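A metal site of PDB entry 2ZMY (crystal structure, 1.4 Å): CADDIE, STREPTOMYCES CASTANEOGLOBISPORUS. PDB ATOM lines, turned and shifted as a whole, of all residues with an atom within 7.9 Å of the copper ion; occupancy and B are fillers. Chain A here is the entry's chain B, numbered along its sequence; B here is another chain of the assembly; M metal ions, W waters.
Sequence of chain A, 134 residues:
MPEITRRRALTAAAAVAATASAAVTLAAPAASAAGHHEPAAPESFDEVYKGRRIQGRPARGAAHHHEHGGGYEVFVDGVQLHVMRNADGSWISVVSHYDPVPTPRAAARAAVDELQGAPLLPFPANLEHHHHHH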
ATOM      1  N   HIS A  66     -11.280  25.629  -0.094  1.00  0.00           N
ATOM      2  CA  HIS A  66     -10.303  25.449   1.000  1.00  0.00           C
ATOM      3  C   HIS A  66     -10.743  24.409   2.015  1.00  0.00           C
ATOM      4  O   HIS A  66     -10.030  23.955   2.913  1.00  0.00           O
ATOM      5  CB  HIS A  66     -10.017  26.811   1.646  1.00  0.00           C
ATOM      6  CG  HIS A  66      -8.750  27.380   1.020  1.00  0.00           C
ATOM      7  ND1 HIS A  66      -8.198  26.758  -0.079  1.00  0.00           N
ATOM      8  CD2 HIS A  66      -7.955  28.425   1.288  1.00  0.00           C
ATOM      9  CE1 HIS A  66      -7.112  27.401  -0.465  1.00  0.00           C
ATOM     10  NE2 HIS A  66      -6.949  28.417   0.349  1.00  0.00           N
ATOM     11  N   GLU A  67     -11.986  23.948   1.875  1.00  0.00           N
ATOM     12  CA  GLU A  67     -12.544  22.976   2.810  1.00  0.00           C
ATOM     13  C   GLU A  67     -13.715  22.324   2.109  1.00  0.00           C
ATOM     14  O   GLU A  67     -14.083  22.835   1.050  1.00  0.00           O
ATOM     15  CB  GLU A  67     -12.908  23.677   4.104  1.00  0.00           C
ATOM     16  CG  GLU A  67     -13.475  25.082   3.847  1.00  0.00           C
ATOM     17  CD  GLU A  67     -14.988  25.035   3.947  1.00  0.00           C
ATOM     18  OE1 GLU A  67     -15.524  23.906   4.005  1.00  0.00           O
ATOM     19  OE2 GLU A  67     -15.618  26.100   3.968  1.00  0.00           O
ATOM     20  N   HIS A  68     -14.306  21.227   2.555  1.00  0.00           N
ATOM     21  CA  HIS A  68     -15.277  20.536   1.721  1.00  0.00           C
ATOM     22  C   HIS A  68     -16.594  21.308   1.632  1.00  0.00           C
ATOM     23  O   HIS A  68     -16.754  22.236   2.411  1.00  0.00           O
ATOM     24  CB  HIS A  68     -15.523  19.126   2.278  1.00  0.00           C
ATOM     25  CG  HIS A  68     -16.430  19.048   3.469  1.00  0.00           C
ATOM     26  ND1 HIS A  68     -16.556  20.074   4.378  1.00  0.00           N
ATOM     27  CD2 HIS A  68     -17.263  18.072   3.897  1.00  0.00           C
ATOM     28  CE1 HIS A  68     -17.423  19.732   5.328  1.00  0.00           C
ATOM     29  NE2 HIS A  68     -17.871  18.507   5.066  1.00  0.00           N
ATOM     30  N   GLY A  69     -17.490  20.918   0.735  1.00  0.00           N
ATOM     31  CA  GLY A  69     -18.850  21.422   0.646  1.00  0.00           C
ATOM     32  C   GLY A  69     -19.833  20.701   1.586  1.00  0.00           C
ATOM     33  O   GLY A  69     -20.477  19.727   1.182  1.00  0.00           O
ATOM     34  N   GLY A  70     -19.942  21.178   2.809  1.00  0.00           N
ATOM     35  CA  GLY A  70     -20.553  20.607   3.970  1.00  0.00           C
ATOM     36  C   GLY A  70     -22.021  20.896   4.195  1.00  0.00           C
ATOM     37  O   GLY A  70     -22.465  22.041   4.109  1.00  0.00           O
ATOM     38  N   GLY A  71     -22.760  19.818   4.495  1.00  0.00           N
ATOM     39  CA  GLY A  71     -24.199  19.862   4.617  1.00  0.00           C
ATOM     40  C   GLY A  71     -24.670  20.267   6.003  1.00  0.00           C
ATOM     41  O   GLY A  71     -25.868  20.261   6.286  1.00  0.00           O
ATOM     42  N   TYR A  72     -23.689  20.569   6.851  1.00  0.00           N
ATOM     43  CA  TYR A  72     -24.099  20.890   8.227  1.00  0.00           C
ATOM     44  C   TYR A  72     -23.133  21.921   8.802  1.00  0.00           C
ATOM     45  O   TYR A  72     -21.923  21.856   8.517  1.00  0.00           O
ATOM     46  CB  TYR A  72     -24.142  19.605   9.065  1.00  0.00           C
ATOM     47  CG  TYR A  72     -24.907  19.761  10.364  1.00  0.00           C
ATOM     48  CD1 TYR A  72     -26.275  19.466  10.414  1.00  0.00           C
ATOM     49  CD2 TYR A  72     -24.271  20.198  11.523  1.00  0.00           C
ATOM     50  CE1 TYR A  72     -26.958  19.616  11.604  1.00  0.00           C
ATOM     51  CE2 TYR A  72     -24.957  20.337  12.693  1.00  0.00           C
ATOM     52  CZ  TYR A  72     -26.317  20.038  12.745  1.00  0.00           C
ATOM     53  OH  TYR A  72     -26.951  20.202  13.954  1.00  0.00           O
ATOM     54  N   GLN A  80     -17.834  29.902  13.247  1.00  0.00           N
ATOM     55  CA  GLN A  80     -18.114  28.608  12.643  1.00  0.00           C
ATOM     56  C   GLN A  80     -16.919  27.680  12.817  1.00  0.00           C
ATOM     57  O   GLN A  80     -15.749  28.053  12.644  1.00  0.00           O
ATOM     58  CB  GLN A  80     -18.481  28.720  11.154  1.00  0.00           C
ATOM     59  CG  GLN A  80     -19.225  27.483  10.647  1.00  0.00           C
ATOM     60  CD  GLN A  80     -19.488  27.580   9.152  1.00  0.00           C
ATOM     61  OE1 GLN A  80     -19.535  26.566   8.440  1.00  0.00           O
ATOM     62  NE2 GLN A  80     -19.648  28.807   8.660  1.00  0.00           N
ATOM     63  N   HIS A  82     -15.369  24.077  11.496  1.00  0.00           N
ATOM     64  CA  HIS A  82     -15.517  23.146  10.391  1.00  0.00           C
ATOM     65  C   HIS A  82     -15.727  21.718  10.930  1.00  0.00           C
ATOM     66  O   HIS A  82     -14.938  21.298  11.755  1.00  0.00           O
ATOM     67  CB  HIS A  82     -14.301  23.122   9.478  1.00  0.00           C
ATOM     68  CG  HIS A  82     -14.583  22.472   8.157  1.00  0.00           C
ATOM     69  ND1 HIS A  82     -14.276  21.145   7.919  1.00  0.00           N
ATOM     70  CD2 HIS A  82     -15.132  22.934   6.999  1.00  0.00           C
ATOM     71  CE1 HIS A  82     -14.625  20.823   6.691  1.00  0.00           C
ATOM     72  NE2 HIS A  82     -15.131  21.879   6.111  1.00  0.00           N
ATOM     73  N   VAL A  83     -16.780  21.087  10.420  1.00  0.00           N
ATOM     74  CA  VAL A  83     -17.088  19.713  10.831  1.00  0.00           C
ATOM     75  C   VAL A  83     -17.337  18.878   9.582  1.00  0.00           C
ATOM     76  O   VAL A  83     -17.616  19.392   8.513  1.00  0.00           O
ATOM     77  CB  VAL A  83     -18.315  19.666  11.762  1.00  0.00           C
ATOM     78  CG1 VAL A  83     -18.029  20.462  13.016  1.00  0.00           C
ATOM     79  CG2 VAL A  83     -19.536  20.237  11.023  1.00  0.00           C
ATOM     80  N   MET A  84     -17.224  17.572   9.741  1.00  0.00           N
ATOM     81  CA  MET A  84     -17.306  16.663   8.624  1.00  0.00           C
ATOM     82  C   MET A  84     -17.925  15.335   9.055  1.00  0.00           C
ATOM     83  O   MET A  84     -17.653  14.862  10.169  1.00  0.00           O
ATOM     84  CB  MET A  84     -15.890  16.432   8.080  1.00  0.00           C
ATOM     85  CG  MET A  84     -15.830  15.253   7.116  1.00  0.00           C
ATOM     86  SD  MET A  84     -14.283  15.234   6.218  1.00  0.00           S
ATOM     87  CE  MET A  84     -13.879  16.973   6.019  1.00  0.00           C
ATOM     88  N   PHE A 123     -12.254  29.471   9.946  1.00  0.00           N
ATOM     89  CA  PHE A 123     -11.504  28.784   8.888  1.00  0.00           C
ATOM     90  C   PHE A 123     -11.641  29.631   7.623  1.00  0.00           C
ATOM     91  O   PHE A 123     -12.693  30.300   7.500  1.00  0.00           O
ATOM     92  CB  PHE A 123     -11.986  27.365   8.637  1.00  0.00           C
ATOM     93  CG  PHE A 123     -13.477  27.236   8.365  1.00  0.00           C
ATOM     94  CD1 PHE A 123     -13.964  27.039   7.091  1.00  0.00           C
ATOM     95  CD2 PHE A 123     -14.391  27.289   9.400  1.00  0.00           C
ATOM     96  CE1 PHE A 123     -15.316  26.904   6.842  1.00  0.00           C
ATOM     97  CE2 PHE A 123     -15.745  27.177   9.149  1.00  0.00           C
ATOM     98  CZ  PHE A 123     -16.218  26.984   7.875  1.00  0.00           C
ATOM     99  N   ILE B  42      -6.887  18.125   4.617  1.00  0.00           N
ATOM    100  CA  ILE B  42      -7.668  17.479   5.683  1.00  0.00           C
ATOM    101  C   ILE B  42      -9.108  17.941   5.678  1.00  0.00           C
ATOM    102  O   ILE B  42     -10.063  17.174   5.889  1.00  0.00           O
ATOM    103  CB  ILE B  42      -7.003  17.793   7.058  1.00  0.00           C
ATOM    104  CG1 ILE B  42      -5.876  16.839   7.425  1.00  0.00           C
ATOM    105  CG2 ILE B  42      -8.003  17.820   8.205  1.00  0.00           C
ATOM    106  CD1 ILE B  42      -6.470  15.599   8.078  1.00  0.00           C
ATOM    107  N   MET B  43      -9.297  19.242   5.458  1.00  0.00           N
ATOM    108  CA  MET B  43     -10.638  19.806   5.483  1.00  0.00           C
ATOM    109  C   MET B  43     -11.441  19.545   4.221  1.00  0.00           C
ATOM    110  O   MET B  43     -12.683  19.599   4.254  1.00  0.00           O
ATOM    111  CB  MET B  43     -10.558  21.325   5.676  1.00  0.00           C
ATOM    112  CG  MET B  43     -10.218  21.686   7.130  1.00  0.00           C
ATOM    113  SD  MET B  43     -10.336  23.479   7.370  1.00  0.00           S
ATOM    114  CE  MET B  43     -10.041  24.054   5.710  1.00  0.00           C
ATOM    115  N   SER B  44     -10.740  19.250   3.108  1.00  0.00           N
ATOM    116  CA  SER B  44     -11.429  19.068   1.829  1.00  0.00           C
ATOM    117  C   SER B  44     -11.707  17.620   1.464  1.00  0.00           C
ATOM    118  O   SER B  44     -12.705  17.337   0.825  1.00  0.00           O
ATOM    119  CB  SER B  44     -10.574  19.672   0.688  1.00  0.00           C
ATOM    120  OG  SER B  44     -10.148  20.951   1.155  1.00  0.00           O
ATOM    121  N   ASP B  45     -10.818  16.699   1.833  1.00  0.00           N
ATOM    122  CA  ASP B  45     -10.990  15.291   1.465  1.00  0.00           C
ATOM    123  C   ASP B  45     -12.303  14.781   2.024  1.00  0.00           C
ATOM    124  O   ASP B  45     -12.476  14.943   3.241  1.00  0.00           O
ATOM    125  CB  ASP B  45      -9.835  14.478   2.039  1.00  0.00           C
ATOM    126  CG  ASP B  45      -8.512  14.666   1.295  1.00  0.00           C
ATOM    127  OD1 ASP B  45      -7.465  14.348   1.902  1.00  0.00           O
ATOM    128  OD2 ASP B  45      -8.487  15.106   0.119  1.00  0.00           O
ATOM    129  N   THR B  46     -13.198  14.174   1.283  1.00  0.00           N
ATOM    130  CA  THR B  46     -14.436  13.669   1.903  1.00  0.00           C
ATOM    131  C   THR B  46     -14.722  12.257   1.412  1.00  0.00           C
ATOM    132  O   THR B  46     -14.325  11.926   0.309  1.00  0.00           O
ATOM    133  CB  THR B  46     -15.726  14.433   1.534  1.00  0.00           C
ATOM    134  OG1 THR B  46     -15.835  14.487   0.097  1.00  0.00           O
ATOM    135  CG2 THR B  46     -15.690  15.851   2.039  1.00  0.00           C
HETATM  136 CU    CU M   1     -16.007  22.080   4.303  1.00  0.00          CU
HETATM  137  O   HOH W   1     -18.192  23.204   5.771  1.00  0.00           O
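The backbone NH of His 68 sits close to the backbone carbonyl oxygen of Met 43 of chain B (2.9 Å).
Of the 17 residues printed, 3 come within 4 Å of the copper ion. Along chain A the residues within 4 Å of the copper ion span positions 67 to 82.
The copper ion is bound by OE1 of Glu 67, NE2 of His 82, O of His 68, ND1 of His 68 and N of His 68.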
